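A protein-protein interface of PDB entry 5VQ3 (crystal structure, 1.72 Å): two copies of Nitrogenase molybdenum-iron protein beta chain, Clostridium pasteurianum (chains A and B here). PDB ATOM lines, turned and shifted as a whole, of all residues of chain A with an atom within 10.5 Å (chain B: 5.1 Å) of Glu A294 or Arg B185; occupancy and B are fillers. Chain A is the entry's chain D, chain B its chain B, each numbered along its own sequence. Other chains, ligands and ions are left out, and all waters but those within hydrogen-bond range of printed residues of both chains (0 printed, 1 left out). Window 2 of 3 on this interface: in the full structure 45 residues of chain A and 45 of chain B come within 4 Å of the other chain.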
ATOM      1  N   ARG A 189     -25.142 -25.185  11.594  1.00  0.00           N
ATOM      2  CA  ARG A 189     -24.371 -25.505  12.806  1.00  0.00           C
ATOM      3  C   ARG A 189     -23.716 -24.245  13.370  1.00  0.00           C
ATOM      4  O   ARG A 189     -23.672 -24.050  14.591  1.00  0.00           O
ATOM      5  CB  ARG A 189     -23.296 -26.594  12.525  1.00  0.00           C
ATOM      6  CG  ARG A 189     -22.627 -27.180  13.771  1.00  0.00           C
ATOM      7  CD  ARG A 189     -21.459 -28.099  13.388  1.00  0.00           C
ATOM      8  NE  ARG A 189     -20.406 -27.310  12.766  1.00  0.00           N
ATOM      9  CZ  ARG A 189     -19.591 -26.500  13.461  1.00  0.00           C
ATOM     10  NH1 ARG A 189     -19.674 -26.438  14.784  1.00  0.00           N
ATOM     11  NH2 ARG A 189     -18.679 -25.759  12.855  1.00  0.00           N
ATOM     12  N   LEU A 190     -23.217 -23.400  12.487  1.00  0.00           N
ATOM     13  CA  LEU A 190     -22.609 -22.141  12.876  1.00  0.00           C
ATOM     14  C   LEU A 190     -23.624 -21.135  13.484  1.00  0.00           C
ATOM     15  O   LEU A 190     -23.295 -20.445  14.448  1.00  0.00           O
ATOM     16  CB  LEU A 190     -21.913 -21.502  11.674  1.00  0.00           C
ATOM     17  CG  LEU A 190     -20.635 -22.258  11.240  1.00  0.00           C
ATOM     18  CD1 LEU A 190     -20.094 -21.694   9.929  1.00  0.00           C
ATOM     19  CD2 LEU A 190     -19.592 -22.228  12.361  1.00  0.00           C
ATOM     20  N   ALA A 193     -24.217 -22.487  16.880  1.00  0.00           N
ATOM     21  CA  ALA A 193     -23.096 -22.266  17.816  1.00  0.00           C
ATOM     22  C   ALA A 193     -23.030 -20.804  18.286  1.00  0.00           C
ATOM     23  O   ALA A 193     -22.576 -20.528  19.395  1.00  0.00           O
ATOM     24  CB  ALA A 193     -21.789 -22.678  17.178  1.00  0.00           C
ATOM     25  N   ASP A 274     -14.905 -15.699   7.575  1.00  0.00           N
ATOM     26  CA  ASP A 274     -14.721 -14.591   8.560  1.00  0.00           C
ATOM     27  C   ASP A 274     -15.833 -13.543   8.323  1.00  0.00           C
ATOM     28  O   ASP A 274     -16.453 -13.080   9.283  1.00  0.00           O
ATOM     29  CB  ASP A 274     -13.359 -13.890   8.386  1.00  0.00           C
ATOM     30  CG  ASP A 274     -12.158 -14.676   8.971  1.00  0.00           C
ATOM     31  OD1 ASP A 274     -12.361 -15.724   9.644  1.00  0.00           O
ATOM     32  OD2 ASP A 274     -11.004 -14.199   8.733  1.00  0.00           O
ATOM     33  N   ILE A 277     -19.153 -14.834   9.648  1.00  0.00           N
ATOM     34  CA  ILE A 277     -19.205 -14.827  11.090  1.00  0.00           C
ATOM     35  C   ILE A 277     -19.371 -13.372  11.565  1.00  0.00           C
ATOM     36  O   ILE A 277     -20.195 -13.083  12.437  1.00  0.00           O
ATOM     37  CB  ILE A 277     -17.946 -15.441  11.693  1.00  0.00           C
ATOM     38  CG1 ILE A 277     -17.890 -16.957  11.391  1.00  0.00           C
ATOM     39  CG2 ILE A 277     -17.919 -15.266  13.207  1.00  0.00           C
ATOM     40  CD1 ILE A 277     -19.066 -17.768  11.874  1.00  0.00           C
ATOM     41  N   VAL A 288     -18.490 -14.173  19.242  1.00  0.00           N
ATOM     42  CA  VAL A 288     -18.064 -15.413  18.600  1.00  0.00           C
ATOM     43  C   VAL A 288     -17.544 -16.376  19.665  1.00  0.00           C
ATOM     44  O   VAL A 288     -16.599 -16.027  20.386  1.00  0.00           O
ATOM     45  CB  VAL A 288     -16.959 -15.158  17.558  1.00  0.00           C
ATOM     46  CG1 VAL A 288     -16.568 -16.466  16.880  1.00  0.00           C
ATOM     47  CG2 VAL A 288     -17.411 -14.121  16.535  1.00  0.00           C
ATOM     48  N   PRO A 289     -18.151 -17.575  19.788  1.00  0.00           N
ATOM     49  CA  PRO A 289     -17.763 -18.538  20.813  1.00  0.00           C
ATOM     50  C   PRO A 289     -16.411 -19.231  20.552  1.00  0.00           C
ATOM     51  O   PRO A 289     -15.926 -19.275  19.413  1.00  0.00           O
ATOM     52  CB  PRO A 289     -18.866 -19.591  20.743  1.00  0.00           C
ATOM     53  CG  PRO A 289     -19.303 -19.566  19.335  1.00  0.00           C
ATOM     54  CD  PRO A 289     -19.235 -18.114  18.943  1.00  0.00           C
ATOM     55  N   ALA A 290     -15.850 -19.800  21.615  1.00  0.00           N
ATOM     56  CA  ALA A 290     -14.506 -20.361  21.590  1.00  0.00           C
ATOM     57  C   ALA A 290     -14.423 -21.518  20.605  1.00  0.00           C
ATOM     58  O   ALA A 290     -13.386 -21.726  19.987  1.00  0.00           O
ATOM     59  CB  ALA A 290     -14.106 -20.818  22.996  1.00  0.00           C
ATOM     60  N   SER A 291     -15.517 -22.274  20.467  1.00  0.00           N
ATOM     61  CA  SER A 291     -15.556 -23.423  19.542  1.00  0.00           C
ATOM     62  C   SER A 291     -15.269 -23.006  18.093  1.00  0.00           C
ATOM     63  O   SER A 291     -14.470 -23.649  17.404  1.00  0.00           O
ATOM     64  CB  SER A 291     -16.886 -24.178  19.628  1.00  0.00           C
ATOM     65  OG  SER A 291     -17.940 -23.407  19.116  1.00  0.00           O
ATOM     66  N   ILE A 292     -15.904 -21.921  17.641  1.00  0.00           N
ATOM     67  CA  ILE A 292     -15.658 -21.406  16.314  1.00  0.00           C
ATOM     68  C   ILE A 292     -14.261 -20.822  16.159  1.00  0.00           C
ATOM     69  O   ILE A 292     -13.595 -21.048  15.138  1.00  0.00           O
ATOM     70  CB  ILE A 292     -16.724 -20.363  15.929  1.00  0.00           C
ATOM     71  CG1 ILE A 292     -18.083 -21.075  15.784  1.00  0.00           C
ATOM     72  CG2 ILE A 292     -16.321 -19.659  14.640  1.00  0.00           C
ATOM     73  CD1 ILE A 292     -19.251 -20.161  15.489  1.00  0.00           C
ATOM     74  N   GLU A 293     -13.796 -20.063  17.163  1.00  0.00           N
ATOM     75  CA  GLU A 293     -12.486 -19.500  17.086  1.00  0.00           C
ATOM     76  C   GLU A 293     -11.434 -20.620  17.044  1.00  0.00           C
ATOM     77  O   GLU A 293     -10.425 -20.479  16.385  1.00  0.00           O
ATOM     78  CB  GLU A 293     -12.238 -18.575  18.287  1.00  0.00           C
ATOM     79  CG  GLU A 293     -10.902 -17.897  18.203  1.00  0.00           C
ATOM     80  CD  GLU A 293     -10.793 -16.662  19.085  1.00  0.00           C
ATOM     81  OE1 GLU A 293     -11.834 -16.052  19.441  1.00  0.00           O
ATOM     82  OE2 GLU A 293      -9.643 -16.309  19.392  1.00  0.00           O
ATOM     83  N   GLU A 294     -11.673 -21.711  17.773  1.00  0.00           N
ATOM     84  CA  GLU A 294     -10.716 -22.839  17.797  1.00  0.00           C
ATOM     85  C   GLU A 294     -10.631 -23.456  16.388  1.00  0.00           C
ATOM     86  O   GLU A 294      -9.535 -23.773  15.908  1.00  0.00           O
ATOM     87  CB  GLU A 294     -11.089 -23.919  18.800  1.00  0.00           C
ATOM     88  CG  GLU A 294     -10.035 -25.011  18.867  1.00  0.00           C
ATOM     89  CD  GLU A 294     -10.394 -26.277  19.612  1.00  0.00           C
ATOM     90  OE1 GLU A 294     -11.554 -26.781  19.563  1.00  0.00           O
ATOM     91  OE2 GLU A 294      -9.452 -26.829  20.241  1.00  0.00           O
ATOM     92  N   GLU A 295     -11.786 -23.642  15.762  1.00  0.00           N
ATOM     93  CA  GLU A 295     -11.829 -24.240  14.423  1.00  0.00           C
ATOM     94  C   GLU A 295     -11.048 -23.366  13.464  1.00  0.00           C
ATOM     95  O   GLU A 295     -10.272 -23.861  12.636  1.00  0.00           O
ATOM     96  CB  GLU A 295     -13.267 -24.401  13.885  1.00  0.00           C
ATOM     97  CG  GLU A 295     -14.238 -25.304  14.630  1.00  0.00           C
ATOM     98  CD  GLU A 295     -15.756 -25.011  14.314  1.00  0.00           C
ATOM     99  OE1 GLU A 295     -16.137 -24.444  13.247  1.00  0.00           O
ATOM    100  OE2 GLU A 295     -16.619 -25.344  15.164  1.00  0.00           O
ATOM    101  N   ARG A 296     -11.280 -22.048  13.513  1.00  0.00           N
ATOM    102  CA  ARG A 296     -10.513 -21.138  12.686  1.00  0.00           C
ATOM    103  C   ARG A 296      -9.013 -21.271  12.894  1.00  0.00           C
ATOM    104  O   ARG A 296      -8.246 -21.342  11.918  1.00  0.00           O
ATOM    105  CB  ARG A 296     -10.954 -19.663  12.888  1.00  0.00           C
ATOM    106  CG  ARG A 296     -10.283 -18.702  11.952  1.00  0.00           C
ATOM    107  CD  ARG A 296     -10.651 -17.246  12.279  1.00  0.00           C
ATOM    108  NE  ARG A 296     -10.174 -16.326  11.276  1.00  0.00           N
ATOM    109  CZ  ARG A 296      -8.936 -15.858  11.197  1.00  0.00           C
ATOM    110  NH1 ARG A 296      -8.013 -16.223  12.082  1.00  0.00           N
ATOM    111  NH2 ARG A 296      -8.617 -15.045  10.224  1.00  0.00           N
ATOM    112  N   GLY A 297      -8.591 -21.294  14.158  1.00  0.00           N
ATOM    113  CA  GLY A 297      -7.192 -21.489  14.521  1.00  0.00           C
ATOM    114  C   GLY A 297      -6.594 -22.798  14.037  1.00  0.00           C
ATOM    115  O   GLY A 297      -5.427 -22.860  13.710  1.00  0.00           O
ATOM    116  N   GLN A 298      -7.396 -23.850  14.013  1.00  0.00           N
ATOM    117  CA  GLN A 298      -6.936 -25.134  13.450  1.00  0.00           C
ATOM    118  C   GLN A 298      -6.764 -25.073  11.931  1.00  0.00           C
ATOM    119  O   GLN A 298      -5.804 -25.627  11.380  1.00  0.00           O
ATOM    120  CB  GLN A 298      -7.926 -26.225  13.789  1.00  0.00           C
ATOM    121  CG  GLN A 298      -7.936 -26.603  15.259  1.00  0.00           C
ATOM    122  CD  GLN A 298      -9.094 -27.523  15.588  1.00  0.00           C
ATOM    123  OE1 GLN A 298     -10.190 -27.348  15.097  1.00  0.00           O
ATOM    124  NE2 GLN A 298      -8.849 -28.512  16.410  1.00  0.00           N
ATOM    125  N   LEU A 299      -7.668 -24.377  11.249  1.00  0.00           N
ATOM    126  CA  LEU A 299      -7.467 -24.090   9.833  1.00  0.00           C
ATOM    127  C   LEU A 299      -6.183 -23.297   9.542  1.00  0.00           C
ATOM    128  O   LEU A 299      -5.390 -23.666   8.666  1.00  0.00           O
ATOM    129  CB  LEU A 299      -8.692 -23.367   9.256  1.00  0.00           C
ATOM    130  CG  LEU A 299      -8.486 -22.805   7.858  1.00  0.00           C
ATOM    131  CD1 LEU A 299      -8.335 -23.966   6.896  1.00  0.00           C
ATOM    132  CD2 LEU A 299      -9.659 -21.941   7.456  1.00  0.00           C
ATOM    133  N   ILE A 300      -5.958 -22.208  10.283  1.00  0.00           N
ATOM    134  CA  ILE A 300      -4.730 -21.464  10.113  1.00  0.00           C
ATOM    135  C   ILE A 300      -3.491 -22.360  10.354  1.00  0.00           C
ATOM    136  O   ILE A 300      -2.504 -22.331   9.599  1.00  0.00           O
ATOM    137  CB  ILE A 300      -4.707 -20.257  11.087  1.00  0.00           C
ATOM    138  CG1 ILE A 300      -5.828 -19.271  10.716  1.00  0.00           C
ATOM    139  CG2 ILE A 300      -3.342 -19.588  11.051  1.00  0.00           C
ATOM    140  CD1 ILE A 300      -5.848 -18.788   9.275  1.00  0.00           C
ATOM    141  N   ASP A 301      -3.573 -23.159  11.404  1.00  0.00           N
ATOM    142  CA  ASP A 301      -2.489 -24.064  11.763  1.00  0.00           C
ATOM    143  C   ASP A 301      -2.182 -25.030  10.615  1.00  0.00           C
ATOM    144  O   ASP A 301      -1.008 -25.246  10.244  1.00  0.00           O
ATOM    145  CB  ASP A 301      -2.842 -24.883  13.020  1.00  0.00           C
ATOM    146  CG  ASP A 301      -1.632 -25.627  13.597  1.00  0.00           C
ATOM    147  OD1 ASP A 301      -0.790 -24.980  14.296  1.00  0.00           O
ATOM    148  OD2 ASP A 301      -1.514 -26.851  13.323  1.00  0.00           O
ATOM    149  N   LEU A 302      -3.246 -25.575  10.035  1.00  0.00           N
ATOM    150  CA  LEU A 302      -3.097 -26.418   8.863  1.00  0.00           C
ATOM    151  C   LEU A 302      -2.505 -25.706   7.633  1.00  0.00           C
ATOM    152  O   LEU A 302      -1.686 -26.278   6.895  1.00  0.00           O
ATOM    153  CB  LEU A 302      -4.438 -27.073   8.518  1.00  0.00           C
ATOM    154  CG  LEU A 302      -4.543 -28.040   7.333  1.00  0.00           C
ATOM    155  CD1 LEU A 302      -3.669 -29.272   7.479  1.00  0.00           C
ATOM    156  CD2 LEU A 302      -5.981 -28.533   7.244  1.00  0.00           C
ATOM    157  N   GLY A 426     -17.309 -22.914   5.560  1.00  0.00           N
ATOM    158  CA  GLY A 426     -16.923 -22.746   6.956  1.00  0.00           C
ATOM    159  C   GLY A 426     -15.481 -23.123   7.200  1.00  0.00           C
ATOM    160  O   GLY A 426     -14.775 -23.508   6.282  1.00  0.00           O
ATOM    161  N   TYR A 427     -15.041 -22.985   8.442  1.00  0.00           N
ATOM    162  CA  TYR A 427     -13.686 -23.357   8.800  1.00  0.00           C
ATOM    163  C   TYR A 427     -13.511 -24.880   8.685  1.00  0.00           C
ATOM    164  O   TYR A 427     -12.460 -25.350   8.209  1.00  0.00           O
ATOM    165  CB  TYR A 427     -13.296 -22.853  10.207  1.00  0.00           C
ATOM    166  CG  TYR A 427     -13.442 -21.354  10.348  1.00  0.00           C
ATOM    167  CD1 TYR A 427     -12.725 -20.485   9.569  1.00  0.00           C
ATOM    168  CD2 TYR A 427     -14.373 -20.829  11.241  1.00  0.00           C
ATOM    169  CE1 TYR A 427     -12.916 -19.104   9.680  1.00  0.00           C
ATOM    170  CE2 TYR A 427     -14.551 -19.472  11.379  1.00  0.00           C
ATOM    171  CZ  TYR A 427     -13.824 -18.600  10.607  1.00  0.00           C
ATOM    172  OH  TYR A 427     -14.017 -17.198  10.723  1.00  0.00           O
ATOM    173  N   LYS A 428     -14.529 -25.626   9.096  1.00  0.00           N
ATOM    174  CA  LYS A 428     -14.521 -27.118   8.956  1.00  0.00           C
ATOM    175  C   LYS A 428     -14.397 -27.575   7.499  1.00  0.00           C
ATOM    176  O   LYS A 428     -13.585 -28.439   7.196  1.00  0.00           O
ATOM    177  CB  LYS A 428     -15.764 -27.747   9.572  1.00  0.00           C
ATOM    178  CG  LYS A 428     -15.676 -27.741  11.081  1.00  0.00           C
ATOM    179  CD  LYS A 428     -16.301 -28.969  11.726  1.00  0.00           C
ATOM    180  CE  LYS A 428     -15.561 -29.263  13.026  1.00  0.00           C
ATOM    181  NZ  LYS A 428     -16.316 -30.210  13.879  1.00  0.00           N
ATOM    182  N   ILE A 431     -10.879 -26.844   6.161  1.00  0.00           N
ATOM    183  CA  ILE A 431      -9.928 -27.896   6.580  1.00  0.00           C
ATOM    184  C   ILE A 431     -10.087 -29.097   5.644  1.00  0.00           C
ATOM    185  O   ILE A 431      -9.131 -29.631   5.181  1.00  0.00           O
ATOM    186  CB  ILE A 431     -10.180 -28.295   8.007  1.00  0.00           C
ATOM    187  CG1 ILE A 431      -9.687 -27.174   8.946  1.00  0.00           C
ATOM    188  CG2 ILE A 431      -9.460 -29.601   8.320  1.00  0.00           C
ATOM    189  CD1 ILE A 431     -10.060 -27.331  10.404  1.00  0.00           C
ATOM    190  N   PRO B 181      -6.665 -37.557  18.992  1.00  0.00           N
ATOM    191  CA  PRO B 181      -7.475 -36.471  19.547  1.00  0.00           C
ATOM    192  C   PRO B 181      -8.797 -36.291  18.829  1.00  0.00           C
ATOM    193  O   PRO B 181      -9.783 -35.953  19.487  1.00  0.00           O
ATOM    194  CB  PRO B 181      -6.574 -35.221  19.407  1.00  0.00           C
ATOM    195  CG  PRO B 181      -5.596 -35.574  18.333  1.00  0.00           C
ATOM    196  CD  PRO B 181      -5.373 -37.066  18.464  1.00  0.00           C
ATOM    197  N   ALA B 182      -8.872 -36.572  17.524  1.00  0.00           N
ATOM    198  CA  ALA B 182     -10.154 -36.422  16.851  1.00  0.00           C
ATOM    199  C   ALA B 182     -11.145 -37.487  17.345  1.00  0.00           C
ATOM    200  O   ALA B 182     -12.358 -37.251  17.375  1.00  0.00           O
ATOM    201  CB  ALA B 182     -10.022 -36.522  15.312  1.00  0.00           C
ATOM    202  N   ASP B 183     -10.629 -38.675  17.641  1.00  0.00           N
ATOM    203  CA  ASP B 183     -11.430 -39.749  18.186  1.00  0.00           C
ATOM    204  C   ASP B 183     -11.932 -39.406  19.557  1.00  0.00           C
ATOM    205  O   ASP B 183     -13.096 -39.690  19.873  1.00  0.00           O
ATOM    206  CB  ASP B 183     -10.649 -41.055  18.194  1.00  0.00           C
ATOM    207  CG  ASP B 183     -10.208 -41.469  16.789  1.00  0.00           C
ATOM    208  OD1 ASP B 183     -11.040 -41.308  15.851  1.00  0.00           O
ATOM    209  OD2 ASP B 183      -9.028 -41.883  16.625  1.00  0.00           O
ATOM    210  N   MET B 184     -11.059 -38.839  20.386  1.00  0.00           N
ATOM    211  CA  MET B 184     -11.457 -38.386  21.683  1.00  0.00           C
ATOM    212  C   MET B 184     -12.585 -37.364  21.550  1.00  0.00           C
ATOM    213  O   MET B 184     -13.551 -37.452  22.293  1.00  0.00           O
ATOM    214  CB  MET B 184     -10.279 -37.840  22.464  1.00  0.00           C
ATOM    215  CG  MET B 184      -9.374 -38.918  23.016  1.00  0.00           C
ATOM    216  SD  MET B 184      -7.640 -38.437  22.995  1.00  0.00           S
ATOM    217  CE  MET B 184      -6.958 -39.893  23.753  1.00  0.00           C
ATOM    218  N   ARG B 185     -12.472 -36.412  20.614  1.00  0.00           N
ATOM    219  CA  ARG B 185     -13.499 -35.381  20.448  1.00  0.00           C
ATOM    220  C   ARG B 185     -14.810 -36.020  20.019  1.00  0.00           C
ATOM    221  O   ARG B 185     -15.875 -35.574  20.417  1.00  0.00           O
ATOM    222  CB  ARG B 185     -13.092 -34.380  19.386  1.00  0.00           C
ATOM    223  CG  ARG B 185     -11.978 -33.414  19.803  1.00  0.00           C
ATOM    224  CD  ARG B 185     -11.689 -32.406  18.696  1.00  0.00           C
ATOM    225  NE  ARG B 185     -10.509 -31.579  18.973  1.00  0.00           N
ATOM    226  CZ  ARG B 185     -10.549 -30.311  19.367  1.00  0.00           C
ATOM    227  NH1 ARG B 185     -11.709 -29.676  19.522  1.00  0.00           N
ATOM    228  NH2 ARG B 185      -9.423 -29.661  19.570  1.00  0.00           N
ATOM    229  N   GLU B 186     -14.753 -37.038  19.164  1.00  0.00           N
ATOM    230  CA  GLU B 186     -15.983 -37.650  18.658  1.00  0.00           C
ATOM    231  C   GLU B 186     -16.657 -38.462  19.778  1.00  0.00           C
ATOM    232  O   GLU B 186     -17.888 -38.465  19.903  1.00  0.00           O
ATOM    233  CB  GLU B 186     -15.721 -38.521  17.437  1.00  0.00           C
ATOM    234  CG  GLU B 186     -16.935 -39.302  16.941  1.00  0.00           C
ATOM    235  CD  GLU B 186     -18.127 -38.424  16.526  1.00  0.00           C
ATOM    236  OE1 GLU B 186     -17.984 -37.197  16.304  1.00  0.00           O
ATOM    237  OE2 GLU B 186     -19.236 -38.995  16.448  1.00  0.00           O
ATOM    238  N   ILE B 187     -15.865 -39.130  20.609  1.00  0.00           N
ATOM    239  CA  ILE B 187     -16.449 -39.856  21.735  1.00  0.00           C
ATOM    240  C   ILE B 187     -17.124 -38.859  22.676  1.00  0.00           C
ATOM    241  O   ILE B 187     -18.263 -39.066  23.106  1.00  0.00           O
ATOM    242  CB  ILE B 187     -15.423 -40.748  22.421  1.00  0.00           C
ATOM    243  CG1 ILE B 187     -15.051 -41.895  21.485  1.00  0.00           C
ATOM    244  CG2 ILE B 187     -15.938 -41.253  23.776  1.00  0.00           C
ATOM    245  CD1 ILE B 187     -13.700 -42.495  21.792  1.00  0.00           C
ATOM    246  N   LYS B 188     -16.464 -37.747  22.943  1.00  0.00           N
ATOM    247  CA  LYS B 188     -17.045 -36.755  23.837  1.00  0.00           C
ATOM    248  C   LYS B 188     -18.331 -36.172  23.214  1.00  0.00           C
ATOM    249  O   LYS B 188     -19.324 -35.952  23.907  1.00  0.00           O
ATOM    250  CB  LYS B 188     -16.056 -35.655  24.148  1.00  0.00           C
ATOM    251  CG  LYS B 188     -14.936 -36.118  25.068  1.00  0.00           C
ATOM    252  CD  LYS B 188     -14.110 -34.938  25.582  1.00  0.00           C
ATOM    253  CE  LYS B 188     -13.347 -34.233  24.492  1.00  0.00           C
ATOM    254  NZ  LYS B 188     -12.537 -33.122  25.026  1.00  0.00           N
ATOM    255  N   ARG B 189     -18.326 -35.939  21.907  1.00  0.00           N
ATOM    256  CA  ARG B 189     -19.526 -35.405  21.275  1.00  0.00           C
ATOM    257  C   ARG B 189     -20.738 -36.356  21.398  1.00  0.00           C
ATOM    258  O   ARG B 189     -21.881 -35.894  21.535  1.00  0.00           O
ATOM    259  CB  ARG B 189     -19.246 -35.085  19.805  1.00  0.00           C
ATOM    260  CG  ARG B 189     -20.397 -34.427  19.063  1.00  0.00           C
ATOM    261  CD  ARG B 189     -20.082 -34.367  17.566  1.00  0.00           C
ATOM    262  NE  ARG B 189     -20.168 -35.680  16.967  1.00  0.00           N
ATOM    263  CZ  ARG B 189     -21.321 -36.265  16.650  1.00  0.00           C
ATOM    264  NH1 ARG B 189     -22.470 -35.618  16.846  1.00  0.00           N
ATOM    265  NH2 ARG B 189     -21.338 -37.476  16.112  1.00  0.00           N
ATOM    266  N   SER B 205      -7.332 -34.115  23.112  1.00  0.00           N
ATOM    267  CA  SER B 205      -7.983 -33.060  22.330  1.00  0.00           C
ATOM    268  C   SER B 205      -7.641 -31.710  22.939  1.00  0.00           C
ATOM    269  O   SER B 205      -7.625 -31.540  24.156  1.00  0.00           O
ATOM    270  CB  SER B 205      -9.502 -33.283  22.241  1.00  0.00           C
ATOM    271  OG  SER B 205     -10.162 -33.242  23.487  1.00  0.00           O
ATOM    272  N   GLY B 206      -7.354 -30.757  22.071  1.00  0.00           N
ATOM    273  CA  GLY B 206      -6.839 -29.464  22.455  1.00  0.00           C
ATOM    274  C   GLY B 206      -5.421 -29.464  22.960  1.00  0.00           C
ATOM    275  O   GLY B 206      -4.951 -28.426  23.474  1.00  0.00           O
ATOM    276  N   ASP B 209      -3.923 -31.328  18.763  1.00  0.00           N
ATOM    277  CA  ASP B 209      -4.631 -30.930  17.545  1.00  0.00           C
ATOM    278  C   ASP B 209      -5.081 -29.484  17.644  1.00  0.00           C
ATOM    279  O   ASP B 209      -6.088 -29.122  17.110  1.00  0.00           O
ATOM    280  CB  ASP B 209      -5.849 -31.844  17.322  1.00  0.00           C
ATOM    281  CG  ASP B 209      -6.880 -31.718  18.455  1.00  0.00           C
ATOM    282  OD1 ASP B 209      -6.554 -31.023  19.440  1.00  0.00           O
ATOM    283  OD2 ASP B 209      -7.986 -32.303  18.377  1.00  0.00           O
ATOM    284  N   GLY B 210      -4.301 -28.663  18.331  1.00  0.00           N
ATOM    285  CA  GLY B 210      -4.712 -27.316  18.642  1.00  0.00           C
ATOM    286  C   GLY B 210      -4.447 -26.261  17.586  1.00  0.00           C
ATOM    287  O   GLY B 210      -3.760 -26.498  16.586  1.00  0.00           O
ATOM    288  N   PRO B 211      -5.011 -25.071  17.807  1.00  0.00           N
ATOM    289  CA  PRO B 211      -4.914 -23.952  16.880  1.00  0.00           C
ATOM    290  C   PRO B 211      -3.599 -23.238  16.967  1.00  0.00           C
ATOM    291  O   PRO B 211      -2.896 -23.378  17.957  1.00  0.00           O
ATOM    292  CB  PRO B 211      -6.044 -22.997  17.356  1.00  0.00           C
ATOM    293  CG  PRO B 211      -6.172 -23.289  18.842  1.00  0.00           C
ATOM    294  CD  PRO B 211      -5.860 -24.772  18.980  1.00  0.00           C
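NE of Arg B185 lies within salt-bridge range of OD2 of Asp B209 (2.7 Å). OD1 of Asp B209 sits at hydrogen-bond distance from N of Gly B206, at 2.8 Å.
Among the printed residues, pairs that only touch across the chains: Glu A294 with Pro B211, Gly A297 with Pro B211, Gln A298 with Pro B211 and Asp A301 with Gly B210.
Of the printed residues of chain B, Gly A297 touches Pro B211. Of the printed residues of chain B, Gln A298 touches Arg B185, Asp B209 and Pro B211. Printed residues of chain B within 4 Å of Asp A301: Gly B210. No residue of chain A comes within 4 Å of Ala B182. Arg B185 touches just these residues of chain A: Glu A294 and Gln A298. No residue of chain A comes within 4 Å of Glu B186. Lys B188 touches none of the printed residues of chain A. No residue of chain A comes within 4 Å of Ser B205. No residue of chain A comes within 4 Å of Gly B206. Of chain A, only Gln A298 (2.9 Å) comes within 4 Å of Asp B209. Of chain A, only Asp A301 (3.8 Å) comes within 4 Å of Gly B210. Of the printed residues of chain A, Pro B211 touches Glu A294 (3.9 Å), Gly A297 (3.4 Å) and Gln A298 (3.7 Å). The nearest residue of chain B that does not touch Glu A294 is Gly B206 (4.3 Å).
1 position is printed for both chains.
NH1 of Arg B185 is in salt-bridge range of OE1 of Glu A294, 2.9 Å away. NH2 of Arg B185 sits close to NE2 of Gln A298, 3.4 Å away. NE2 of Gln A298 sits at hydrogen-bond distance from O of Asp B209 (2.9 Å).
Printed residues of chain B that touch a printed residue of chain A: Arg B185, Asp B209, Gly B210 and Pro B211. Hydrophobic or aromatic side chains of chain B within 4 Å of the printed part of chain A: Pro B211. Of the 24 printed residues of chain A, 4 touch a printed residue of chain B. Among the printed residues, 7 pairs touch across the chains.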
